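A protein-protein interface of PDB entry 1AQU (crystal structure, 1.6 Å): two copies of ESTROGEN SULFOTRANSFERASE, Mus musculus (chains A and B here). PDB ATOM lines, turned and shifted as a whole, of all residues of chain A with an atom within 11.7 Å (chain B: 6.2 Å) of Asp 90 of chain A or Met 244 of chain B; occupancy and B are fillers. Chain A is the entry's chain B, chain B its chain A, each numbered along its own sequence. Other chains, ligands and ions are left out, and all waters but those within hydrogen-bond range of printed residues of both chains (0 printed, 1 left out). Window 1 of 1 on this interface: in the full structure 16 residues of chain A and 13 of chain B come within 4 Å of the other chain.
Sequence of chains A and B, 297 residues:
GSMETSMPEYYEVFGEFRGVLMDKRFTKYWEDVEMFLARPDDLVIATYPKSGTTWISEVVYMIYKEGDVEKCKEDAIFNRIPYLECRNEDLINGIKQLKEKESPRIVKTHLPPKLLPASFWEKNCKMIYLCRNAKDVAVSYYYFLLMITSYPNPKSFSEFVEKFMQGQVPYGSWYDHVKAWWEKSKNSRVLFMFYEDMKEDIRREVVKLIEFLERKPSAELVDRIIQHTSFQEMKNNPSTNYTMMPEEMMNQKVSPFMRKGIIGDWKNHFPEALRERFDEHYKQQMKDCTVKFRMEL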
ATOM      1  N   LYS A  24       2.496  10.178  16.772  1.00  0.00           N
ATOM      2  CA  LYS A  24       3.047  11.167  15.839  1.00  0.00           C
ATOM      3  C   LYS A  24       3.425  12.513  16.471  1.00  0.00           C
ATOM      4  O   LYS A  24       4.301  13.220  15.968  1.00  0.00           O
ATOM      5  CB  LYS A  24       2.073  11.375  14.668  1.00  0.00           C
ATOM      6  CG  LYS A  24       1.934  10.147  13.760  1.00  0.00           C
ATOM      7  CD  LYS A  24       1.098  10.429  12.514  1.00  0.00           C
ATOM      8  CE  LYS A  24       0.609   9.138  11.854  1.00  0.00           C
ATOM      9  NZ  LYS A  24      -0.476   9.376  10.848  1.00  0.00           N
ATOM     10  N   ARG A  25       2.783  12.867  17.580  1.00  0.00           N
ATOM     11  CA  ARG A  25       3.092  14.123  18.247  1.00  0.00           C
ATOM     12  C   ARG A  25       4.509  14.100  18.835  1.00  0.00           C
ATOM     13  O   ARG A  25       5.134  15.159  19.014  1.00  0.00           O
ATOM     14  CB  ARG A  25       2.064  14.402  19.355  1.00  0.00           C
ATOM     15  CG  ARG A  25       0.662  14.782  18.850  1.00  0.00           C
ATOM     16  CD  ARG A  25      -0.357  14.833  20.007  1.00  0.00           C
ATOM     17  NE  ARG A  25      -0.691  13.496  20.519  1.00  0.00           N
ATOM     18  CZ  ARG A  25      -1.843  13.172  21.104  1.00  0.00           C
ATOM     19  NH1 ARG A  25      -2.796  14.082  21.263  1.00  0.00           N
ATOM     20  NH2 ARG A  25      -2.044  11.928  21.523  1.00  0.00           N
ATOM     21  N   PHE A  26       5.017  12.898  19.131  1.00  0.00           N
ATOM     22  CA  PHE A  26       6.358  12.728  19.699  1.00  0.00           C
ATOM     23  C   PHE A  26       7.460  12.592  18.624  1.00  0.00           C
ATOM     24  O   PHE A  26       8.656  12.578  18.957  1.00  0.00           O
ATOM     25  CB  PHE A  26       6.432  11.476  20.607  1.00  0.00           C
ATOM     26  CG  PHE A  26       5.482  11.484  21.790  1.00  0.00           C
ATOM     27  CD1 PHE A  26       4.704  12.598  22.103  1.00  0.00           C
ATOM     28  CD2 PHE A  26       5.365  10.345  22.590  1.00  0.00           C
ATOM     29  CE1 PHE A  26       3.818  12.575  23.193  1.00  0.00           C
ATOM     30  CE2 PHE A  26       4.485  10.302  23.678  1.00  0.00           C
ATOM     31  CZ  PHE A  26       3.712  11.419  23.983  1.00  0.00           C
ATOM     32  N   LYS A  28       7.049  14.372  15.396  1.00  0.00           N
ATOM     33  CA  LYS A  28       6.960  15.532  14.503  1.00  0.00           C
ATOM     34  C   LYS A  28       8.230  16.397  14.567  1.00  0.00           C
ATOM     35  O   LYS A  28       8.729  16.862  13.534  1.00  0.00           O
ATOM     36  CB  LYS A  28       5.734  16.383  14.858  1.00  0.00           C
ATOM     37  CG  LYS A  28       5.628  17.673  14.052  1.00  0.00           C
ATOM     38  CD  LYS A  28       4.320  18.395  14.346  1.00  0.00           C
ATOM     39  CE  LYS A  28       4.160  19.626  13.468  1.00  0.00           C
ATOM     40  NZ  LYS A  28       2.757  20.136  13.493  1.00  0.00           N
ATOM     41  N   TYR A  29       8.750  16.596  15.778  1.00  0.00           N
ATOM     42  CA  TYR A  29       9.956  17.399  16.004  1.00  0.00           C
ATOM     43  C   TYR A  29      11.097  16.510  16.523  1.00  0.00           C
ATOM     44  O   TYR A  29      11.825  16.892  17.449  1.00  0.00           O
ATOM     45  CB  TYR A  29       9.668  18.526  17.018  1.00  0.00           C
ATOM     46  CG  TYR A  29       8.490  19.416  16.647  1.00  0.00           C
ATOM     47  CD1 TYR A  29       8.609  20.377  15.649  1.00  0.00           C
ATOM     48  CD2 TYR A  29       7.252  19.275  17.271  1.00  0.00           C
ATOM     49  CE1 TYR A  29       7.521  21.176  15.278  1.00  0.00           C
ATOM     50  CE2 TYR A  29       6.156  20.069  16.904  1.00  0.00           C
ATOM     51  CZ  TYR A  29       6.302  21.015  15.906  1.00  0.00           C
ATOM     52  OH  TYR A  29       5.231  21.804  15.526  1.00  0.00           O
ATOM     53  N   ASP A  32      14.761  17.552  17.786  1.00  0.00           N
ATOM     54  CA  ASP A  32      15.011  18.081  19.130  1.00  0.00           C
ATOM     55  C   ASP A  32      15.487  16.972  20.081  1.00  0.00           C
ATOM     56  O   ASP A  32      16.263  17.224  21.014  1.00  0.00           O
ATOM     57  CB  ASP A  32      13.731  18.724  19.707  1.00  0.00           C
ATOM     58  CG  ASP A  32      13.318  20.015  18.978  1.00  0.00           C
ATOM     59  OD1 ASP A  32      14.037  20.439  18.044  1.00  0.00           O
ATOM     60  OD2 ASP A  32      12.267  20.603  19.337  1.00  0.00           O
ATOM     61  N   GLU A  85      11.018  12.572  25.668  1.00  0.00           N
ATOM     62  CA  GLU A  85      10.417  12.702  24.349  1.00  0.00           C
ATOM     63  C   GLU A  85       8.951  13.142  24.285  1.00  0.00           C
ATOM     64  O   GLU A  85       8.398  13.299  23.188  1.00  0.00           O
ATOM     65  CB  GLU A  85      10.594  11.388  23.582  1.00  0.00           C
ATOM     66  CG  GLU A  85       9.744  10.229  24.101  1.00  0.00           C
ATOM     67  CD  GLU A  85      10.436   9.371  25.175  1.00  0.00           C
ATOM     68  OE1 GLU A  85      11.505   9.765  25.693  1.00  0.00           O
ATOM     69  OE2 GLU A  85       9.882   8.290  25.500  1.00  0.00           O
ATOM     70  N   CYS A  86       8.323  13.347  25.443  1.00  0.00           N
ATOM     71  CA  CYS A  86       6.918  13.777  25.462  1.00  0.00           C
ATOM     72  C   CYS A  86       6.787  15.188  24.868  1.00  0.00           C
ATOM     73  O   CYS A  86       7.505  16.105  25.259  1.00  0.00           O
ATOM     74  CB  CYS A  86       6.370  13.762  26.896  1.00  0.00           C
ATOM     75  SG  CYS A  86       4.550  13.866  26.984  1.00  0.00           S
ATOM     76  N   ARG A  87       5.859  15.352  23.934  1.00  0.00           N
ATOM     77  CA  ARG A  87       5.662  16.628  23.257  1.00  0.00           C
ATOM     78  C   ARG A  87       4.250  16.752  22.682  1.00  0.00           C
ATOM     79  O   ARG A  87       3.739  15.824  22.068  1.00  0.00           O
ATOM     80  CB  ARG A  87       6.709  16.750  22.127  1.00  0.00           C
ATOM     81  CG  ARG A  87       6.564  17.960  21.193  1.00  0.00           C
ATOM     82  CD  ARG A  87       7.137  19.222  21.832  1.00  0.00           C
ATOM     83  NE  ARG A  87       7.130  20.371  20.925  1.00  0.00           N
ATOM     84  CZ  ARG A  87       8.189  20.773  20.229  1.00  0.00           C
ATOM     85  NH1 ARG A  87       9.338  20.120  20.334  1.00  0.00           N
ATOM     86  NH2 ARG A  87       8.101  21.822  19.419  1.00  0.00           N
ATOM     87  N   ASN A  88       3.611  17.897  22.920  1.00  0.00           N
ATOM     88  CA  ASN A  88       2.272  18.196  22.382  1.00  0.00           C
ATOM     89  C   ASN A  88       2.344  19.679  21.997  1.00  0.00           C
ATOM     90  O   ASN A  88       1.931  20.563  22.755  1.00  0.00           O
ATOM     91  CB  ASN A  88       1.160  17.962  23.423  1.00  0.00           C
ATOM     92  CG  ASN A  88      -0.197  17.648  22.778  1.00  0.00           C
ATOM     93  OD1 ASN A  88      -0.450  18.018  21.626  1.00  0.00           O
ATOM     94  ND2 ASN A  88      -1.069  16.960  23.513  1.00  0.00           N
ATOM     95  N   GLU A  89       2.896  19.925  20.810  1.00  0.00           N
ATOM     96  CA  GLU A  89       3.099  21.261  20.273  1.00  0.00           C
ATOM     97  C   GLU A  89       3.773  22.145  21.324  1.00  0.00           C
ATOM     98  O   GLU A  89       4.800  21.755  21.878  1.00  0.00           O
ATOM     99  CB  GLU A  89       1.769  21.864  19.794  1.00  0.00           C
ATOM    100  CG  GLU A  89       1.235  21.276  18.472  1.00  0.00           C
ATOM    101  CD  GLU A  89       2.256  21.261  17.326  1.00  0.00           C
ATOM    102  OE1 GLU A  89       3.275  21.985  17.383  1.00  0.00           O
ATOM    103  OE2 GLU A  89       2.035  20.515  16.348  1.00  0.00           O
ATOM    104  N   ASP A  90       3.209  23.319  21.617  1.00  0.00           N
ATOM    105  CA  ASP A  90       3.825  24.225  22.591  1.00  0.00           C
ATOM    106  C   ASP A  90       3.285  24.160  24.016  1.00  0.00           C
ATOM    107  O   ASP A  90       3.745  24.904  24.883  1.00  0.00           O
ATOM    108  CB  ASP A  90       3.748  25.672  22.090  1.00  0.00           C
ATOM    109  CG  ASP A  90       4.731  25.952  20.965  1.00  0.00           C
ATOM    110  OD1 ASP A  90       5.557  25.064  20.663  1.00  0.00           O
ATOM    111  OD2 ASP A  90       4.682  27.051  20.373  1.00  0.00           O
ATOM    112  N   LEU A  91       2.315  23.283  24.260  1.00  0.00           N
ATOM    113  CA  LEU A  91       1.741  23.124  25.593  1.00  0.00           C
ATOM    114  C   LEU A  91       2.581  22.198  26.487  1.00  0.00           C
ATOM    115  O   LEU A  91       2.727  22.449  27.684  1.00  0.00           O
ATOM    116  CB  LEU A  91       0.323  22.573  25.493  1.00  0.00           C
ATOM    117  CG  LEU A  91      -0.330  22.343  26.858  1.00  0.00           C
ATOM    118  CD1 LEU A  91      -0.480  23.688  27.563  1.00  0.00           C
ATOM    119  CD2 LEU A  91      -1.681  21.637  26.697  1.00  0.00           C
ATOM    120  N   ILE A  92       3.108  21.117  25.904  1.00  0.00           N
ATOM    121  CA  ILE A  92       3.955  20.161  26.636  1.00  0.00           C
ATOM    122  C   ILE A  92       5.249  19.952  25.843  1.00  0.00           C
ATOM    123  O   ILE A  92       5.200  19.668  24.650  1.00  0.00           O
ATOM    124  CB  ILE A  92       3.246  18.776  26.816  1.00  0.00           C
ATOM    125  CG1 ILE A  92       1.976  18.932  27.657  1.00  0.00           C
ATOM    126  CG2 ILE A  92       4.192  17.773  27.505  1.00  0.00           C
ATOM    127  CD1 ILE A  92       1.110  17.683  27.692  1.00  0.00           C
ATOM    128  N   ASN A  93       6.394  20.082  26.509  1.00  0.00           N
ATOM    129  CA  ASN A  93       7.695  19.917  25.854  1.00  0.00           C
ATOM    130  C   ASN A  93       8.752  19.453  26.871  1.00  0.00           C
ATOM    131  O   ASN A  93       9.329  20.272  27.589  1.00  0.00           O
ATOM    132  CB  ASN A  93       8.116  21.260  25.218  1.00  0.00           C
ATOM    133  CG  ASN A  93       9.306  21.138  24.267  1.00  0.00           C
ATOM    134  OD1 ASN A  93       9.425  21.910  23.310  1.00  0.00           O
ATOM    135  ND2 ASN A  93      10.194  20.182  24.530  1.00  0.00           N
ATOM    136  N   GLY A  94       9.005  18.142  26.916  1.00  0.00           N
ATOM    137  CA  GLY A  94       9.995  17.592  27.839  1.00  0.00           C
ATOM    138  C   GLY A  94      11.434  18.054  27.649  1.00  0.00           C
ATOM    139  O   GLY A  94      12.165  18.226  28.622  1.00  0.00           O
ATOM    140  N   ILE A  95      11.844  18.251  26.396  1.00  0.00           N
ATOM    141  CA  ILE A  95      13.200  18.715  26.074  1.00  0.00           C
ATOM    142  C   ILE A  95      13.441  20.107  26.672  1.00  0.00           C
ATOM    143  O   ILE A  95      14.481  20.366  27.272  1.00  0.00           O
ATOM    144  CB  ILE A  95      13.420  18.808  24.532  1.00  0.00           C
ATOM    145  CG1 ILE A  95      13.305  17.417  23.883  1.00  0.00           C
ATOM    146  CG2 ILE A  95      14.774  19.439  24.242  1.00  0.00           C
ATOM    147  CD1 ILE A  95      14.456  16.476  24.221  1.00  0.00           C
ATOM    148  N   LYS A  96      12.466  20.996  26.504  1.00  0.00           N
ATOM    149  CA  LYS A  96      12.567  22.359  27.013  1.00  0.00           C
ATOM    150  C   LYS A  96      12.665  22.345  28.530  1.00  0.00           C
ATOM    151  O   LYS A  96      13.442  23.085  29.122  1.00  0.00           O
ATOM    152  CB  LYS A  96      11.350  23.169  26.569  1.00  0.00           C
ATOM    153  CG  LYS A  96      11.092  24.403  27.414  1.00  0.00           C
ATOM    154  CD  LYS A  96      10.429  25.492  26.596  1.00  0.00           C
ATOM    155  CE  LYS A  96      11.461  26.295  25.799  1.00  0.00           C
ATOM    156  NZ  LYS A  96      12.873  26.011  26.207  1.00  0.00           N
ATOM    157  N   GLN A  97      11.867  21.498  29.161  1.00  0.00           N
ATOM    158  CA  GLN A  97      11.903  21.371  30.616  1.00  0.00           C
ATOM    159  C   GLN A  97      13.315  20.973  31.073  1.00  0.00           C
ATOM    160  O   GLN A  97      13.838  21.496  32.059  1.00  0.00           O
ATOM    161  CB  GLN A  97      10.951  20.270  31.075  1.00  0.00           C
ATOM    162  CG  GLN A  97       9.526  20.680  31.335  1.00  0.00           C
ATOM    163  CD  GLN A  97       8.709  19.521  31.877  1.00  0.00           C
ATOM    164  OE1 GLN A  97       8.519  19.392  33.088  1.00  0.00           O
ATOM    165  NE2 GLN A  97       8.229  18.662  30.982  1.00  0.00           N
ATOM    166  N   LYS A  99      16.213  21.417  29.524  1.00  0.00           N
ATOM    167  CA  LYS A  99      17.211  22.451  29.282  1.00  0.00           C
ATOM    168  C   LYS A  99      17.195  23.475  30.422  1.00  0.00           C
ATOM    169  O   LYS A  99      18.216  24.090  30.725  1.00  0.00           O
ATOM    170  CB  LYS A  99      16.946  23.156  27.945  1.00  0.00           C
ATOM    171  CG  LYS A  99      17.472  22.410  26.721  1.00  0.00           C
ATOM    172  CD  LYS A  99      16.702  22.795  25.468  1.00  0.00           C
ATOM    173  CE  LYS A  99      17.444  22.377  24.200  1.00  0.00           C
ATOM    174  NZ  LYS A  99      16.558  22.393  22.983  1.00  0.00           N
ATOM    175  N   GLU A 100      16.041  23.641  31.057  1.00  0.00           N
ATOM    176  CA  GLU A 100      15.904  24.601  32.147  1.00  0.00           C
ATOM    177  C   GLU A 100      16.062  23.971  33.533  1.00  0.00           C
ATOM    178  O   GLU A 100      15.944  24.656  34.555  1.00  0.00           O
ATOM    179  CB  GLU A 100      14.543  25.299  32.051  1.00  0.00           C
ATOM    180  CG  GLU A 100      14.355  26.093  30.765  1.00  0.00           C
ATOM    181  CD  GLU A 100      12.887  26.318  30.409  1.00  0.00           C
ATOM    182  OE1 GLU A 100      12.014  25.989  31.239  1.00  0.00           O
ATOM    183  OE2 GLU A 100      12.607  26.827  29.296  1.00  0.00           O
ATOM    184  N   MET A 249      -7.314  15.325  29.195  1.00  0.00           N
ATOM    185  CA  MET A 249      -6.212  14.581  28.587  1.00  0.00           C
ATOM    186  C   MET A 249      -6.184  13.129  29.073  1.00  0.00           C
ATOM    187  O   MET A 249      -6.058  12.193  28.272  1.00  0.00           O
ATOM    188  CB  MET A 249      -4.885  15.256  28.923  1.00  0.00           C
ATOM    189  CG  MET A 249      -4.724  16.642  28.315  1.00  0.00           C
ATOM    190  SD  MET A 249      -3.018  17.189  28.434  1.00  0.00           S
ATOM    191  CE  MET A 249      -2.870  18.111  26.905  1.00  0.00           C
ATOM    192  N   ASP B  75       7.203  30.985  18.681  1.00  0.00           N
ATOM    193  CA  ASP B  75       6.679  30.580  20.022  1.00  0.00           C
ATOM    194  C   ASP B  75       5.237  31.053  20.174  1.00  0.00           C
ATOM    195  O   ASP B  75       4.919  32.191  19.830  1.00  0.00           O
ATOM    196  CB  ASP B  75       7.542  31.186  21.127  1.00  0.00           C
ATOM    197  CG  ASP B  75       7.492  30.388  22.403  1.00  0.00           C
ATOM    198  OD1 ASP B  75       6.955  29.255  22.393  1.00  0.00           O
ATOM    199  OD2 ASP B  75       7.988  30.898  23.423  1.00  0.00           O
ATOM    200  N   ALA B  76       4.376  30.177  20.690  1.00  0.00           N
ATOM    201  CA  ALA B  76       2.961  30.493  20.866  1.00  0.00           C
ATOM    202  C   ALA B  76       2.769  31.815  21.602  1.00  0.00           C
ATOM    203  O   ALA B  76       3.541  32.151  22.508  1.00  0.00           O
ATOM    204  CB  ALA B  76       2.261  29.364  21.616  1.00  0.00           C
ATOM    205  N   PHE B  78       0.616  32.557  23.790  1.00  0.00           N
ATOM    206  CA  PHE B  78       0.321  32.338  25.208  1.00  0.00           C
ATOM    207  C   PHE B  78       1.573  32.008  26.026  1.00  0.00           C
ATOM    208  O   PHE B  78       1.505  31.858  27.247  1.00  0.00           O
ATOM    209  CB  PHE B  78      -0.763  31.258  25.401  1.00  0.00           C
ATOM    210  CG  PHE B  78      -0.488  29.961  24.685  1.00  0.00           C
ATOM    211  CD1 PHE B  78       0.480  29.079  25.165  1.00  0.00           C
ATOM    212  CD2 PHE B  78      -1.206  29.616  23.545  1.00  0.00           C
ATOM    213  CE1 PHE B  78       0.735  27.859  24.517  1.00  0.00           C
ATOM    214  CE2 PHE B  78      -0.967  28.404  22.881  1.00  0.00           C
ATOM    215  CZ  PHE B  78       0.011  27.522  23.374  1.00  0.00           C
ATOM    216  N   ASN B  79       2.714  31.916  25.342  1.00  0.00           N
ATOM    217  CA  ASN B  79       3.999  31.663  25.987  1.00  0.00           C
ATOM    218  C   ASN B  79       4.775  32.984  26.052  1.00  0.00           C
ATOM    219  O   ASN B  79       5.441  33.280  27.047  1.00  0.00           O
ATOM    220  CB  ASN B  79       4.812  30.616  25.203  1.00  0.00           C
ATOM    221  CG  ASN B  79       4.439  29.182  25.583  1.00  0.00           C
ATOM    222  OD1 ASN B  79       3.863  28.937  26.642  1.00  0.00           O
ATOM    223  ND2 ASN B  79       4.762  28.233  24.710  1.00  0.00           N
ATOM    224  N   PRO B 238       0.289  30.185  12.843  1.00  0.00           N
ATOM    225  CA  PRO B 238       0.103  29.175  13.898  1.00  0.00           C
ATOM    226  C   PRO B 238       0.422  29.649  15.323  1.00  0.00           C
ATOM    227  O   PRO B 238      -0.031  29.053  16.306  1.00  0.00           O
ATOM    228  CB  PRO B 238       1.008  28.023  13.468  1.00  0.00           C
ATOM    229  CG  PRO B 238       2.002  28.645  12.528  1.00  0.00           C
ATOM    230  CD  PRO B 238       1.281  29.760  11.839  1.00  0.00           C
ATOM    231  N   SER B 239       1.208  30.717  15.426  1.00  0.00           N
ATOM    232  CA  SER B 239       1.586  31.275  16.715  1.00  0.00           C
ATOM    233  C   SER B 239       0.433  32.041  17.350  1.00  0.00           C
ATOM    234  O   SER B 239       0.303  32.082  18.575  1.00  0.00           O
ATOM    235  CB  SER B 239       2.775  32.222  16.539  1.00  0.00           C
ATOM    236  OG  SER B 239       3.076  32.908  17.736  1.00  0.00           O
ATOM    237  N   ASN B 241      -3.103  31.833  15.974  1.00  0.00           N
ATOM    238  CA  ASN B 241      -4.435  31.262  15.764  1.00  0.00           C
ATOM    239  C   ASN B 241      -4.850  30.118  16.728  1.00  0.00           C
ATOM    240  O   ASN B 241      -5.882  29.457  16.520  1.00  0.00           O
ATOM    241  CB  ASN B 241      -4.620  30.819  14.298  1.00  0.00           C
ATOM    242  CG  ASN B 241      -3.709  29.653  13.914  1.00  0.00           C
ATOM    243  OD1 ASN B 241      -3.504  29.399  12.728  1.00  0.00           O
ATOM    244  ND2 ASN B 241      -3.148  28.922  14.858  1.00  0.00           N
ATOM    245  N   TYR B 242      -4.059  29.935  17.760  1.00  0.00           N
ATOM    246  CA  TYR B 242      -4.318  28.975  18.867  1.00  0.00           C
ATOM    247  C   TYR B 242      -4.416  27.485  18.410  1.00  0.00           C
ATOM    248  O   TYR B 242      -5.111  26.675  19.056  1.00  0.00           O
ATOM    249  CB  TYR B 242      -5.605  29.374  19.617  1.00  0.00           C
ATOM    250  CG  TYR B 242      -5.337  30.409  20.726  1.00  0.00           C
ATOM    251  CD1 TYR B 242      -5.372  31.781  20.436  1.00  0.00           C
ATOM    252  CD2 TYR B 242      -5.045  29.987  22.033  1.00  0.00           C
ATOM    253  CE1 TYR B 242      -5.108  32.723  21.442  1.00  0.00           C
ATOM    254  CE2 TYR B 242      -4.779  30.929  23.037  1.00  0.00           C
ATOM    255  CZ  TYR B 242      -4.809  32.295  22.742  1.00  0.00           C
ATOM    256  OH  TYR B 242      -4.547  33.210  23.715  1.00  0.00           O
ATOM    257  N   THR B 243      -3.692  27.147  17.311  1.00  0.00           N
ATOM    258  CA  THR B 243      -3.578  25.731  16.798  1.00  0.00           C
ATOM    259  C   THR B 243      -2.453  25.032  17.587  1.00  0.00           C
ATOM    260  O   THR B 243      -2.271  23.811  17.484  1.00  0.00           O
ATOM    261  CB  THR B 243      -3.280  25.664  15.295  1.00  0.00           C
ATOM    262  OG1 THR B 243      -2.143  26.442  14.979  1.00  0.00           O
ATOM    263  CG2 THR B 243      -4.442  26.158  14.432  1.00  0.00           C
ATOM    264  N   MET B 244      -1.705  25.817  18.370  1.00  0.00           N
ATOM    265  CA  MET B 244      -0.616  25.293  19.207  1.00  0.00           C
ATOM    266  C   MET B 244      -1.181  24.776  20.538  1.00  0.00           C
ATOM    267  O   MET B 244      -0.434  24.302  21.408  1.00  0.00           O
ATOM    268  CB  MET B 244       0.429  26.379  19.505  1.00  0.00           C
ATOM    269  CG  MET B 244       1.287  26.796  18.319  1.00  0.00           C
ATOM    270  SD  MET B 244       2.348  25.472  17.696  1.00  0.00           S
ATOM    271  CE  MET B 244       1.257  24.680  16.489  1.00  0.00           C
ATOM    272  N   MET B 245      -2.498  24.889  20.690  1.00  0.00           N
ATOM    273  CA  MET B 245      -3.199  24.431  21.885  1.00  0.00           C
ATOM    274  C   MET B 245      -4.013  23.200  21.470  1.00  0.00           C
ATOM    275  O   MET B 245      -4.779  23.254  20.513  1.00  0.00           O
ATOM    276  CB  MET B 245      -4.119  25.549  22.402  1.00  0.00           C
ATOM    277  CG  MET B 245      -4.924  25.200  23.642  1.00  0.00           C
ATOM    278  SD  MET B 245      -3.943  25.173  25.163  1.00  0.00           S
ATOM    279  CE  MET B 245      -3.261  26.803  25.164  1.00  0.00           C
ATOM    280  N   PRO B 246      -3.835  22.064  22.175  1.00  0.00           N
ATOM    281  CA  PRO B 246      -4.527  20.789  21.916  1.00  0.00           C
ATOM    282  C   PRO B 246      -6.040  20.838  21.691  1.00  0.00           C
ATOM    283  O   PRO B 246      -6.775  21.486  22.445  1.00  0.00           O
ATOM    284  CB  PRO B 246      -4.176  19.931  23.130  1.00  0.00           C
ATOM    285  CG  PRO B 246      -2.868  20.456  23.570  1.00  0.00           C
ATOM    286  CD  PRO B 246      -2.896  21.947  23.303  1.00  0.00           C
ATOM    287  N   GLN B 252     -11.288  23.473  17.569  1.00  0.00           N
ATOM    288  CA  GLN B 252     -11.593  24.423  16.508  1.00  0.00           C
ATOM    289  C   GLN B 252     -12.331  23.809  15.326  1.00  0.00           C
ATOM    290  O   GLN B 252     -12.633  24.488  14.344  1.00  0.00           O
ATOM    291  CB  GLN B 252     -10.302  25.133  16.064  1.00  0.00           C
ATOM    292  CG  GLN B 252      -9.668  25.947  17.203  1.00  0.00           C
ATOM    293  CD  GLN B 252      -8.682  27.005  16.732  1.00  0.00           C
ATOM    294  OE1 GLN B 252      -8.930  27.715  15.760  1.00  0.00           O
ATOM    295  NE2 GLN B 252      -7.557  27.116  17.432  1.00  0.00           N
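The side-chain carboxylate (OD2) of Asp 90 of chain A sits at hydrogen-bond distance from the backbone NH (N) of Ala 76 of chain B (3.2 Å). The side-chain amide nitrogen (ND2) of Asn 79 of chain B is in hydrogen-bond range of the backbone carbonyl oxygen (O) of Asp 90 of chain A, 3.5 Å away. OE1 of Glu 89 of chain A sits close to SD of Met 244 of chain B.
OD1 of Asp 75 of chain B lies within hydrogen-bond range of ND2 of Asn 79 of chain B, 3.3 Å away. The side-chain hydroxyl of Ser 239 of chain B lies within hydrogen-bond range of the backbone carbonyl oxygen of Asp 75 of chain B (2.9 Å). The side-chain amino group (NZ) of Lys 28 of chain A lies within salt-bridge range of the side-chain carboxylate (OE2) of Glu 89 of chain A (3.0 Å). The side-chain hydroxyl (OH) of Tyr 29 of chain A sits at hydrogen-bond distance from the side-chain carboxylate (OE1) of Glu 89 of chain A (2.7 Å). The backbone carbonyl oxygen (O) of Glu 89 of chain A is in hydrogen-bond range of the guanidinium group (NE) of Arg 87 of chain A (2.9 Å).
Among the printed residues, merely in contact across the chains: Asn 88 of chain A with Pro 246 of chain B, Asp 90 of chain A with Asp 75 of chain B, Asp 90 of chain A with Met 244 of chain B and Leu 91 of chain A with Pro 246 of chain B.
Printed residues of chain B within 4 Å of Asn 88 of chain A: Pro 246. Of the printed residues of chain B, Glu 89 of chain A touches Met 244 (3.5 Å). Asp 90 of chain A touches just these residues of chain B: Asp 75 (3.8 Å), Ala 76 (3.2 Å), Asn 79 (3.5 Å) and Met 244 (3.8 Å). Printed residues of chain B within 4 Å of Leu 91 of chain A: Pro 246 (3.5 Å). Of the printed residues of chain A, Asp 75 of chain B touches Asp 90 (3.8 Å). Ala 76 of chain B touches just one residue of chain A: Asp 90. Phe 78 of chain B touches none of the printed residues of chain A. Of the printed residues of chain A, Asn 79 of chain B touches Asp 90 (3.5 Å). No residue of chain A comes within 4 Å of Pro 238 of chain B. No residue of chain A comes within 4 Å of Ser 239 of chain B. No residue of chain A comes within 4 Å of Asn 241 of chain B. No residue of chain A comes within 4 Å of Thr 243 of chain B. Met 244 of chain B touches just these residues of chain A: Glu 89 (3.5 Å) and Asp 90 (3.8 Å). Pro 246 of chain B touches two residues of chain A. The nearest residue of chain A that does not touch Met 244 of chain B is Leu 91 of chain A (4.1 Å).
Of the 22 printed residues of chain A, 4 touch a printed residue of chain B. Of the 13 printed residues of chain B, 5 touch a printed residue of chain A. Printed residues of chain B that touch a printed residue of chain A: Asp 75, Ala 76, Asn 79, Met 244 and Pro 246. Among the printed residues, 7 pairs touch across the chains. Among the printed residues, no Asp or Glu carboxylate lies within 4 Å of a Lys or Arg side-chain nitrogen of the other chain.
No position is printed for both chains.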
